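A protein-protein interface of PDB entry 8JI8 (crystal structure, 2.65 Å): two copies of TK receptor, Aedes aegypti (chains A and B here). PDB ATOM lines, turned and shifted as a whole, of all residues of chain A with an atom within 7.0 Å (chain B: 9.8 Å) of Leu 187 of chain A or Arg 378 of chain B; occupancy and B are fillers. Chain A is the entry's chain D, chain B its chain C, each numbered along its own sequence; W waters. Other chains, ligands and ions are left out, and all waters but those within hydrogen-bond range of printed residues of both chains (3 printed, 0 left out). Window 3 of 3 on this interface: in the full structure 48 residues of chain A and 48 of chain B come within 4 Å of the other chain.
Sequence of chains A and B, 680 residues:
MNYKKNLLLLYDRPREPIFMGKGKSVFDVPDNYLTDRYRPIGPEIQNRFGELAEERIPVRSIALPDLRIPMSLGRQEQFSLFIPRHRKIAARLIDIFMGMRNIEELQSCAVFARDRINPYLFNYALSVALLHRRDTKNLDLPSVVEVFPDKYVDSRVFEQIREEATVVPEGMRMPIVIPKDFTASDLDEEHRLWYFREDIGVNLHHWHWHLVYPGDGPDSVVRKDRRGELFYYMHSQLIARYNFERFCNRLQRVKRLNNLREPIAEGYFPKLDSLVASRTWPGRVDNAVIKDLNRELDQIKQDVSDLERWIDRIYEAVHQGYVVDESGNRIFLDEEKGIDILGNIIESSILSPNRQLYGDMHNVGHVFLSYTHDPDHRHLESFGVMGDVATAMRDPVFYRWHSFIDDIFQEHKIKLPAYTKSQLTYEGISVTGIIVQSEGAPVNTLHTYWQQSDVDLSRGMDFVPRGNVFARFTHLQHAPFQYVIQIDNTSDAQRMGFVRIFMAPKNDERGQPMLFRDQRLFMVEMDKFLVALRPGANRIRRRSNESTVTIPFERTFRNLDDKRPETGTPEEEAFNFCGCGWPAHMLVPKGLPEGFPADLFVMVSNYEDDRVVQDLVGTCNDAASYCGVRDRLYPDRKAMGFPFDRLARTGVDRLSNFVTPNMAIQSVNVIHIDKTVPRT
The backbone carbonyl oxygen (O) of Arg 378 of chain B lies within hydrogen-bond range of the backbone NH (N) of Ser 185 of chain A, at 2.8 Å.
The backbone carbonyl oxygen of Leu 187 of chain A is in hydrogen-bond range of the guanidinium group of Arg 378 of chain B.
The guanidinium group of Arg 378 of chain B lies within salt-bridge range of the side-chain carboxylate of Asp 286 of chain A, at 3.8 Å.
The backbone carbonyl oxygen (O) of His 379 of chain B sits at hydrogen-bond distance from the side-chain amino group (NZ) of Lys 271 of chain A (2.6 Å).
The side-chain carboxylate of Asp 286 of chain A lies within hydrogen-bond range of a ring nitrogen (NE2) of His 379 of chain B, at 3.3 Å.
OE2 of Glu 381 of chain B lies within salt-bridge range of NZ of Lys 271 of chain A, at 3.1 Å.
The backbone carbonyl oxygen (O) of Thr 183 of chain A sits close to the backbone carbonyl oxygen (O) of His 379 of chain B (3.3 Å).
NH2 of Arg 295 of chain B lies within hydrogen-bond range of O of Glu 381 of chain B (2.9 Å).
N of Leu 380 of chain B is in hydrogen-bond range of OD2 of Asp 374 of chain B (3.4 Å).
The side-chain carboxylate (OD2) of Asp 374 of chain B lies within hydrogen-bond range of the backbone NH (N) of Glu 381 of chain B (3.0 Å).
O of Thr 183 of chain A sits at hydrogen-bond distance from NZ of Lys 271 of chain A (3.1 Å).
The side-chain hydroxyl (OG) of Ser 185 of chain A sits at hydrogen-bond distance from the backbone NH (N) of Leu 187 of chain A, 3.0 Å away.
N of Gly 267 of chain A is in hydrogen-bond range of OD1 of Asp 286 of chain A, 2.8 Å away.
Among the printed residues, pairs that only touch across the chains: Ala 184 of chain A with Arg 378 of chain B (3.2 Å), Ala 184 of chain A with Leu 380 of chain B (3.6 Å), Ser 185 of chain A with Leu 380 of chain B (3.9 Å), Leu 187 of chain A with Asp 376 of chain B (3.2 Å), Gly 267 of chain A with His 379 of chain B (3.6 Å) and Lys 271 of chain A with Leu 380 of chain B (3.2 Å).
Printed residues of chain B within 4 Å of Thr 183 of chain A: His 379 (3.3 Å).
Ala 184 of chain A touches just these residues of chain B: Arg 378 (3.2 Å) and Leu 380 (3.6 Å).
No residue of chain B comes within 4 Å of Asp 188 of chain A.
Arg 295 of chain B touches none of the printed residues of chain A.
His 377 of chain B touches none of the printed residues of chain A.
Arg 378 of chain B touches four residues of chain A.
Of the printed residues of chain A, Leu 380 of chain B touches Ala 184, Ser 185 and Lys 271.
The nearest residue of chain A that does not touch Arg 378 of chain B is Asp 188 of chain A (4.03 Å).
The nearest printed residue of chain A that does not touch Glu 381 of chain B is Thr 183 of chain A (6.1 Å).
Hydrophobic or aromatic side chains of chain B that line the printed part of chain A: His 379 and Leu 380.
Of the 12 printed residues of chain A, 7 touch a printed residue of chain B.
Hydrophobic or aromatic side chains of chain A within 4 Å of the printed part of chain B: Ala 184 and Leu 187.
Among the printed residues, 13 pairs touch across the chains.
No position is printed for both chains.
Water W2 bridges the backbone carbonyl oxygen of Thr 183 of chain A (2.6 Å) and a ring nitrogen (ND1) of His 379 of chain B (2.9 Å).
Water W3 bridges O of His 373 of chain B (2.6 Å) and N of Asp 286 of chain A (3.0 Å).
Water W1 bridges N of Lys 271 of chain A and OE2 of Glu 381 of chain B.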
ATOM      1  N   THR A 183      -5.839   7.154   9.797  1.00  0.00           N
ATOM      2  CA  THR A 183      -5.886   6.339   8.601  1.00  0.00           C
ATOM      3  C   THR A 183      -4.549   6.362   7.866  1.00  0.00           C
ATOM      4  O   THR A 183      -4.316   5.528   6.987  1.00  0.00           O
ATOM      5  CB  THR A 183      -7.042   6.779   7.705  1.00  0.00           C
ATOM      6  OG1 THR A 183      -6.770   8.130   7.340  1.00  0.00           O
ATOM      7  CG2 THR A 183      -8.380   6.656   8.400  1.00  0.00           C
ATOM      8  N   ALA A 184      -3.660   7.283   8.243  1.00  0.00           N
ATOM      9  CA  ALA A 184      -2.439   7.458   7.481  1.00  0.00           C
ATOM     10  C   ALA A 184      -1.463   8.386   8.202  1.00  0.00           C
ATOM     11  O   ALA A 184      -1.871   9.272   8.943  1.00  0.00           O
ATOM     12  CB  ALA A 184      -2.799   7.984   6.120  1.00  0.00           C
ATOM     13  N   SER A 185      -0.168   8.159   7.962  1.00  0.00           N
ATOM     14  CA  SER A 185       0.902   8.934   8.565  1.00  0.00           C
ATOM     15  C   SER A 185       1.215  10.138   7.684  1.00  0.00           C
ATOM     16  O   SER A 185       0.761  10.195   6.548  1.00  0.00           O
ATOM     17  CB  SER A 185       2.135   8.102   8.722  1.00  0.00           C
ATOM     18  OG  SER A 185       2.898   8.202   7.534  1.00  0.00           O
ATOM     19  N   ASP A 186       2.074  11.032   8.199  1.00  0.00           N
ATOM     20  CA  ASP A 186       2.489  12.239   7.501  1.00  0.00           C
ATOM     21  C   ASP A 186       3.374  11.911   6.302  1.00  0.00           C
ATOM     22  O   ASP A 186       3.597  12.781   5.468  1.00  0.00           O
ATOM     23  CB  ASP A 186       3.123  13.255   8.455  1.00  0.00           C
ATOM     24  CG  ASP A 186       4.297  12.750   9.281  1.00  0.00           C
ATOM     25  OD1 ASP A 186       4.930  11.732   8.880  1.00  0.00           O
ATOM     26  OD2 ASP A 186       4.568  13.377  10.336  1.00  0.00           O
ATOM     27  N   LEU A 187       3.813  10.653   6.169  1.00  0.00           N
ATOM     28  CA  LEU A 187       4.448  10.186   4.939  1.00  0.00           C
ATOM     29  C   LEU A 187       3.516  10.360   3.732  1.00  0.00           C
ATOM     30  O   LEU A 187       3.997  10.416   2.598  1.00  0.00           O
ATOM     31  CB  LEU A 187       4.849   8.711   5.077  1.00  0.00           C
ATOM     32  CG  LEU A 187       5.865   8.363   6.165  1.00  0.00           C
ATOM     33  CD1 LEU A 187       6.212   6.885   6.104  1.00  0.00           C
ATOM     34  CD2 LEU A 187       7.130   9.210   6.053  1.00  0.00           C
ATOM     35  N   ASP A 188       2.194  10.387   3.979  1.00  0.00           N
ATOM     36  CA  ASP A 188       1.176  10.658   2.967  1.00  0.00           C
ATOM     37  C   ASP A 188       0.558  12.039   3.223  1.00  0.00           C
ATOM     38  O   ASP A 188      -0.009  12.276   4.290  1.00  0.00           O
ATOM     39  CB  ASP A 188       0.123   9.544   2.982  1.00  0.00           C
ATOM     40  CG  ASP A 188      -1.081   9.761   2.081  1.00  0.00           C
ATOM     41  OD1 ASP A 188      -1.015  10.651   1.193  1.00  0.00           O
ATOM     42  OD2 ASP A 188      -2.087   9.042   2.290  1.00  0.00           O
ATOM     43  N   GLU A 189       0.688  12.952   2.246  1.00  0.00           N
ATOM     44  CA  GLU A 189       0.297  14.351   2.422  1.00  0.00           C
ATOM     45  C   GLU A 189      -1.222  14.484   2.536  1.00  0.00           C
ATOM     46  O   GLU A 189      -1.709  15.392   3.215  1.00  0.00           O
ATOM     47  CB  GLU A 189       0.840  15.242   1.300  1.00  0.00           C
ATOM     48  CG  GLU A 189       0.448  14.859  -0.126  1.00  0.00           C
ATOM     49  CD  GLU A 189       1.175  15.641  -1.215  1.00  0.00           C
ATOM     50  OE1 GLU A 189       0.635  15.754  -2.331  1.00  0.00           O
ATOM     51  OE2 GLU A 189       2.287  16.142  -0.955  1.00  0.00           O
ATOM     52  N   GLU A 190      -1.953  13.532   1.932  1.00  0.00           N
ATOM     53  CA  GLU A 190      -3.400  13.514   1.996  1.00  0.00           C
ATOM     54  C   GLU A 190      -3.937  13.403   3.422  1.00  0.00           C
ATOM     55  O   GLU A 190      -5.068  13.796   3.682  1.00  0.00           O
ATOM     56  CB  GLU A 190      -3.919  12.354   1.158  1.00  0.00           C
ATOM     57  CG  GLU A 190      -3.712  12.580  -0.322  1.00  0.00           C
ATOM     58  CD  GLU A 190      -4.331  13.842  -0.903  1.00  0.00           C
ATOM     59  OE1 GLU A 190      -3.875  14.235  -1.975  1.00  0.00           O
ATOM     60  OE2 GLU A 190      -5.300  14.396  -0.316  1.00  0.00           O
ATOM     61  N   HIS A 191      -3.128  12.901   4.350  1.00  0.00           N
ATOM     62  CA  HIS A 191      -3.572  12.657   5.706  1.00  0.00           C
ATOM     63  C   HIS A 191      -4.041  13.960   6.352  1.00  0.00           C
ATOM     64  O   HIS A 191      -4.828  13.933   7.291  1.00  0.00           O
ATOM     65  CB  HIS A 191      -2.460  12.010   6.543  1.00  0.00           C
ATOM     66  CG  HIS A 191      -1.630  12.983   7.345  1.00  0.00           C
ATOM     67  ND1 HIS A 191      -1.907  13.286   8.667  1.00  0.00           N
ATOM     68  CD2 HIS A 191      -0.563  13.754   7.014  1.00  0.00           C
ATOM     69  CE1 HIS A 191      -1.033  14.191   9.110  1.00  0.00           C
ATOM     70  NE2 HIS A 191      -0.197  14.480   8.130  1.00  0.00           N
ATOM     71  N   GLY A 267      -3.492   5.541  -2.567  1.00  0.00           N
ATOM     72  CA  GLY A 267      -4.119   4.452  -1.834  1.00  0.00           C
ATOM     73  C   GLY A 267      -4.882   4.972  -0.621  1.00  0.00           C
ATOM     74  O   GLY A 267      -4.736   6.135  -0.260  1.00  0.00           O
ATOM     75  N   LYS A 271      -9.575   1.608   8.065  1.00  0.00           N
ATOM     76  CA  LYS A 271      -9.564   1.149   9.450  1.00  0.00           C
ATOM     77  C   LYS A 271     -10.980   0.969  10.017  1.00  0.00           C
ATOM     78  O   LYS A 271     -11.145   0.968  11.240  1.00  0.00           O
ATOM     79  CB  LYS A 271      -8.821   2.129  10.366  1.00  0.00           C
ATOM     80  CG  LYS A 271      -7.487   2.656   9.852  1.00  0.00           C
ATOM     81  CD  LYS A 271      -6.390   1.629   9.761  1.00  0.00           C
ATOM     82  CE  LYS A 271      -5.065   2.259   9.387  1.00  0.00           C
ATOM     83  NZ  LYS A 271      -5.038   2.627   7.956  1.00  0.00           N
ATOM     84  N   ASP A 286      -1.582   1.799  -3.039  1.00  0.00           N
ATOM     85  CA  ASP A 286      -1.111   2.819  -3.959  1.00  0.00           C
ATOM     86  C   ASP A 286      -0.953   2.179  -5.345  1.00  0.00           C
ATOM     87  O   ASP A 286      -0.731   0.971  -5.459  1.00  0.00           O
ATOM     88  CB  ASP A 286       0.205   3.452  -3.482  1.00  0.00           C
ATOM     89  CG  ASP A 286       0.127   4.213  -2.169  1.00  0.00           C
ATOM     90  OD1 ASP A 286      -0.859   4.971  -1.988  1.00  0.00           O
ATOM     91  OD2 ASP A 286       1.078   4.088  -1.350  1.00  0.00           O
ATOM     92  N   LYS B 291       7.982  -5.243  -2.171  1.00  0.00           N
ATOM     93  CA  LYS B 291       8.459  -3.868  -2.201  1.00  0.00           C
ATOM     94  C   LYS B 291       9.512  -3.702  -1.110  1.00  0.00           C
ATOM     95  O   LYS B 291       9.439  -4.381  -0.090  1.00  0.00           O
ATOM     96  CB  LYS B 291       7.326  -2.877  -1.916  1.00  0.00           C
ATOM     97  CG  LYS B 291       6.152  -2.857  -2.888  1.00  0.00           C
ATOM     98  CD  LYS B 291       6.340  -1.915  -4.056  1.00  0.00           C
ATOM     99  CE  LYS B 291       6.260  -0.446  -3.691  1.00  0.00           C
ATOM    100  NZ  LYS B 291       6.726   0.423  -4.801  1.00  0.00           N
ATOM    101  N   ASP B 292      10.462  -2.779  -1.319  1.00  0.00           N
ATOM    102  CA  ASP B 292      11.471  -2.473  -0.313  1.00  0.00           C
ATOM    103  C   ASP B 292      10.760  -2.009   0.953  1.00  0.00           C
ATOM    104  O   ASP B 292       9.718  -1.370   0.868  1.00  0.00           O
ATOM    105  CB  ASP B 292      12.451  -1.384  -0.767  1.00  0.00           C
ATOM    106  CG  ASP B 292      13.402  -1.709  -1.915  1.00  0.00           C
ATOM    107  OD1 ASP B 292      13.299  -2.783  -2.545  1.00  0.00           O
ATOM    108  OD2 ASP B 292      14.262  -0.862  -2.166  1.00  0.00           O
ATOM    109  N   LEU B 293      11.348  -2.287   2.117  1.00  0.00           N
ATOM    110  CA  LEU B 293      10.664  -2.095   3.378  1.00  0.00           C
ATOM    111  C   LEU B 293      11.307  -0.985   4.185  1.00  0.00           C
ATOM    112  O   LEU B 293      12.515  -1.045   4.422  1.00  0.00           O
ATOM    113  CB  LEU B 293      10.782  -3.391   4.167  1.00  0.00           C
ATOM    114  CG  LEU B 293       9.918  -4.526   3.662  1.00  0.00           C
ATOM    115  CD1 LEU B 293      10.186  -5.769   4.488  1.00  0.00           C
ATOM    116  CD2 LEU B 293       8.459  -4.114   3.721  1.00  0.00           C
ATOM    117  N   ASN B 294      10.466  -0.061   4.676  1.00  0.00           N
ATOM    118  CA  ASN B 294      10.888   0.981   5.606  1.00  0.00           C
ATOM    119  C   ASN B 294       9.793   1.270   6.642  1.00  0.00           C
ATOM    120  O   ASN B 294       8.973   2.173   6.442  1.00  0.00           O
ATOM    121  CB  ASN B 294      11.298   2.243   4.852  1.00  0.00           C
ATOM    122  CG  ASN B 294      11.966   3.269   5.740  1.00  0.00           C
ATOM    123  OD1 ASN B 294      12.033   3.127   6.962  1.00  0.00           O
ATOM    124  ND2 ASN B 294      12.480   4.314   5.121  1.00  0.00           N
ATOM    125  N   ARG B 295       9.827   0.517   7.761  1.00  0.00           N
ATOM    126  CA  ARG B 295       8.847   0.625   8.838  1.00  0.00           C
ATOM    127  C   ARG B 295       9.563   0.936  10.157  1.00  0.00           C
ATOM    128  O   ARG B 295      10.117   0.046  10.813  1.00  0.00           O
ATOM    129  CB  ARG B 295       8.062  -0.675   9.044  1.00  0.00           C
ATOM    130  CG  ARG B 295       7.751  -1.510   7.814  1.00  0.00           C
ATOM    131  CD  ARG B 295       6.283  -1.546   7.433  1.00  0.00           C
ATOM    132  NE  ARG B 295       5.413  -1.979   8.513  1.00  0.00           N
ATOM    133  CZ  ARG B 295       4.113  -1.716   8.559  1.00  0.00           C
ATOM    134  NH1 ARG B 295       3.463  -1.327   7.474  1.00  0.00           N
ATOM    135  NH2 ARG B 295       3.453  -1.852   9.688  1.00  0.00           N
ATOM    136  N   GLU B 296       9.533   2.212  10.552  1.00  0.00           N
ATOM    137  CA  GLU B 296      10.316   2.714  11.675  1.00  0.00           C
ATOM    138  C   GLU B 296       9.913   2.068  12.998  1.00  0.00           C
ATOM    139  O   GLU B 296      10.796   1.662  13.751  1.00  0.00           O
ATOM    140  CB  GLU B 296      10.203   4.235  11.738  1.00  0.00           C
ATOM    141  CG  GLU B 296      11.102   4.887  10.705  1.00  0.00           C
ATOM    142  CD  GLU B 296      11.003   6.393  10.622  1.00  0.00           C
ATOM    143  OE1 GLU B 296      11.014   6.920   9.486  1.00  0.00           O
ATOM    144  OE2 GLU B 296      10.885   7.019  11.694  1.00  0.00           O
ATOM    145  N   LEU B 297       8.598   1.983  13.266  1.00  0.00           N
ATOM    146  CA  LEU B 297       8.090   1.395  14.496  1.00  0.00           C
ATOM    147  C   LEU B 297       8.536  -0.057  14.590  1.00  0.00           C
ATOM    148  O   LEU B 297       8.956  -0.473  15.670  1.00  0.00           O
ATOM    149  CB  LEU B 297       6.561   1.515  14.574  1.00  0.00           C
ATOM    150  CG  LEU B 297       5.879   0.940  15.828  1.00  0.00           C
ATOM    151  CD1 LEU B 297       6.342   1.637  17.099  1.00  0.00           C
ATOM    152  CD2 LEU B 297       4.354   1.023  15.727  1.00  0.00           C
ATOM    153  N   TYR B 371       3.822  -7.650   3.839  1.00  0.00           N
ATOM    154  CA  TYR B 371       3.661  -6.201   3.910  1.00  0.00           C
ATOM    155  C   TYR B 371       3.656  -5.548   2.519  1.00  0.00           C
ATOM    156  O   TYR B 371       3.924  -4.365   2.392  1.00  0.00           O
ATOM    157  CB  TYR B 371       4.804  -5.611   4.744  1.00  0.00           C
ATOM    158  CG  TYR B 371       4.610  -5.460   6.246  1.00  0.00           C
ATOM    159  CD1 TYR B 371       3.467  -4.869   6.780  1.00  0.00           C
ATOM    160  CD2 TYR B 371       5.632  -5.798   7.131  1.00  0.00           C
ATOM    161  CE1 TYR B 371       3.325  -4.668   8.150  1.00  0.00           C
ATOM    162  CE2 TYR B 371       5.501  -5.596   8.498  1.00  0.00           C
ATOM    163  CZ  TYR B 371       4.341  -5.038   9.015  1.00  0.00           C
ATOM    164  OH  TYR B 371       4.205  -4.855  10.372  1.00  0.00           O
ATOM    165  N   HIS B 373       1.457  -4.480   0.895  1.00  0.00           N
ATOM    166  CA  HIS B 373       0.369  -3.533   0.774  1.00  0.00           C
ATOM    167  C   HIS B 373       0.683  -2.208   1.468  1.00  0.00           C
ATOM    168  O   HIS B 373       0.007  -1.211   1.193  1.00  0.00           O
ATOM    169  CB  HIS B 373      -0.897  -4.130   1.379  1.00  0.00           C
ATOM    170  CG  HIS B 373      -0.741  -4.446   2.829  1.00  0.00           C
ATOM    171  ND1 HIS B 373      -0.111  -5.580   3.284  1.00  0.00           N
ATOM    172  CD2 HIS B 373      -1.114  -3.742   3.915  1.00  0.00           C
ATOM    173  CE1 HIS B 373      -0.121  -5.553   4.613  1.00  0.00           C
ATOM    174  NE2 HIS B 373      -0.726  -4.448   5.017  1.00  0.00           N
ATOM    175  N   ASP B 374       1.675  -2.201   2.379  1.00  0.00           N
ATOM    176  CA  ASP B 374       2.010  -0.986   3.104  1.00  0.00           C
ATOM    177  C   ASP B 374       3.475  -1.034   3.563  1.00  0.00           C
ATOM    178  O   ASP B 374       3.800  -1.008   4.758  1.00  0.00           O
ATOM    179  CB  ASP B 374       0.976  -0.746   4.203  1.00  0.00           C
ATOM    180  CG  ASP B 374       1.257   0.478   5.053  1.00  0.00           C
ATOM    181  OD1 ASP B 374       1.651   1.499   4.470  1.00  0.00           O
ATOM    182  OD2 ASP B 374       1.074   0.408   6.295  1.00  0.00           O
ATOM    183  N   PRO B 375       4.428  -1.011   2.608  1.00  0.00           N
ATOM    184  CA  PRO B 375       5.832  -1.236   2.933  1.00  0.00           C
ATOM    185  C   PRO B 375       6.578  -0.117   3.670  1.00  0.00           C
ATOM    186  O   PRO B 375       7.648  -0.394   4.223  1.00  0.00           O
ATOM    187  CB  PRO B 375       6.450  -1.570   1.558  1.00  0.00           C
ATOM    188  CG  PRO B 375       5.571  -0.874   0.544  1.00  0.00           C
ATOM    189  CD  PRO B 375       4.190  -0.851   1.163  1.00  0.00           C
ATOM    190  N   ASP B 376       6.043   1.116   3.736  1.00  0.00           N
ATOM    191  CA  ASP B 376       6.700   2.135   4.568  1.00  0.00           C
ATOM    192  C   ASP B 376       5.780   2.696   5.661  1.00  0.00           C
ATOM    193  O   ASP B 376       6.084   3.727   6.259  1.00  0.00           O
ATOM    194  CB  ASP B 376       7.303   3.271   3.739  1.00  0.00           C
ATOM    195  CG  ASP B 376       6.285   4.012   2.891  1.00  0.00           C
ATOM    196  OD1 ASP B 376       5.071   3.979   3.242  1.00  0.00           O
ATOM    197  OD2 ASP B 376       6.703   4.587   1.860  1.00  0.00           O
ATOM    198  N   HIS B 377       4.672   2.002   5.937  1.00  0.00           N
ATOM    199  CA  HIS B 377       3.808   2.304   7.065  1.00  0.00           C
ATOM    200  C   HIS B 377       3.061   3.628   6.894  1.00  0.00           C
ATOM    201  O   HIS B 377       2.426   4.088   7.844  1.00  0.00           O
ATOM    202  CB  HIS B 377       4.583   2.270   8.388  1.00  0.00           C
ATOM    203  CG  HIS B 377       3.733   1.958   9.579  1.00  0.00           C
ATOM    204  ND1 HIS B 377       2.568   1.202   9.519  1.00  0.00           N
ATOM    205  CD2 HIS B 377       3.932   2.243  10.875  1.00  0.00           C
ATOM    206  CE1 HIS B 377       2.056   1.077  10.736  1.00  0.00           C
ATOM    207  NE2 HIS B 377       2.866   1.703  11.578  1.00  0.00           N
ATOM    208  N   ARG B 378       3.066   4.208   5.687  1.00  0.00           N
ATOM    209  CA  ARG B 378       2.309   5.432   5.434  1.00  0.00           C
ATOM    210  C   ARG B 378       0.813   5.203   5.665  1.00  0.00           C
ATOM    211  O   ARG B 378       0.124   6.119   6.087  1.00  0.00           O
ATOM    212  CB  ARG B 378       2.553   6.002   4.028  1.00  0.00           C
ATOM    213  CG  ARG B 378       1.782   5.310   2.914  1.00  0.00           C
ATOM    214  CD  ARG B 378       1.926   5.959   1.550  1.00  0.00           C
ATOM    215  NE  ARG B 378       3.309   5.996   1.105  1.00  0.00           N
ATOM    216  CZ  ARG B 378       3.922   7.091   0.675  1.00  0.00           C
ATOM    217  NH1 ARG B 378       3.229   8.207   0.512  1.00  0.00           N
ATOM    218  NH2 ARG B 378       5.214   7.056   0.390  1.00  0.00           N
ATOM    219  N   HIS B 379       0.302   3.994   5.427  1.00  0.00           N
ATOM    220  CA  HIS B 379      -1.113   3.716   5.633  1.00  0.00           C
ATOM    221  C   HIS B 379      -1.428   3.128   7.015  1.00  0.00           C
ATOM    222  O   HIS B 379      -2.571   2.760   7.267  1.00  0.00           O
ATOM    223  CB  HIS B 379      -1.618   2.782   4.533  1.00  0.00           C
ATOM    224  CG  HIS B 379      -1.518   3.387   3.190  1.00  0.00           C
ATOM    225  ND1 HIS B 379      -2.229   4.519   2.849  1.00  0.00           N
ATOM    226  CD2 HIS B 379      -0.815   3.020   2.102  1.00  0.00           C
ATOM    227  CE1 HIS B 379      -1.954   4.823   1.581  1.00  0.00           C
ATOM    228  NE2 HIS B 379      -1.092   3.924   1.109  1.00  0.00           N
ATOM    229  N   LEU B 380      -0.435   3.044   7.903  1.00  0.00           N
ATOM    230  CA  LEU B 380      -0.604   2.583   9.282  1.00  0.00           C
ATOM    231  C   LEU B 380      -1.340   1.250   9.351  1.00  0.00           C
ATOM    232  O   LEU B 380      -2.207   1.092  10.210  1.00  0.00           O
ATOM    233  CB  LEU B 380      -1.350   3.642  10.099  1.00  0.00           C
ATOM    234  CG  LEU B 380      -0.640   4.985  10.238  1.00  0.00           C
ATOM    235  CD1 LEU B 380      -1.529   6.020  10.910  1.00  0.00           C
ATOM    236  CD2 LEU B 380       0.652   4.833  11.016  1.00  0.00           C
ATOM    237  N   GLU B 381      -0.951   0.305   8.478  1.00  0.00           N
ATOM    238  CA  GLU B 381      -1.515  -1.038   8.446  1.00  0.00           C
ATOM    239  C   GLU B 381      -0.527  -2.090   8.975  1.00  0.00           C
ATOM    240  O   GLU B 381       0.684  -1.973   8.836  1.00  0.00           O
ATOM    241  CB  GLU B 381      -1.902  -1.394   7.013  1.00  0.00           C
ATOM    242  CG  GLU B 381      -3.114  -0.649   6.493  1.00  0.00           C
ATOM    243  CD  GLU B 381      -4.436  -1.214   6.973  1.00  0.00           C
ATOM    244  OE1 GLU B 381      -4.539  -2.456   6.998  1.00  0.00           O
ATOM    245  OE2 GLU B 381      -5.357  -0.423   7.312  1.00  0.00           O
ATOM    246  N   SER B 382      -1.066  -3.170   9.553  1.00  0.00           N
ATOM    247  CA  SER B 382      -0.262  -4.264  10.077  1.00  0.00           C
ATOM    248  C   SER B 382       0.033  -5.290   8.973  1.00  0.00           C
ATOM    249  O   SER B 382      -0.302  -5.099   7.812  1.00  0.00           O
ATOM    250  CB  SER B 382      -0.951  -4.880  11.261  1.00  0.00           C
ATOM    251  OG  SER B 382      -0.215  -6.002  11.713  1.00  0.00           O
HETATM  252  O   HOH W   1      -8.118  -0.226   6.478  1.00  0.00           O
HETATM  253  O   HOH W   2      -4.599   5.171   4.387  1.00  0.00           O
HETATM  254  O   HOH W   3      -0.138   0.659  -0.666  1.00  0.00           O
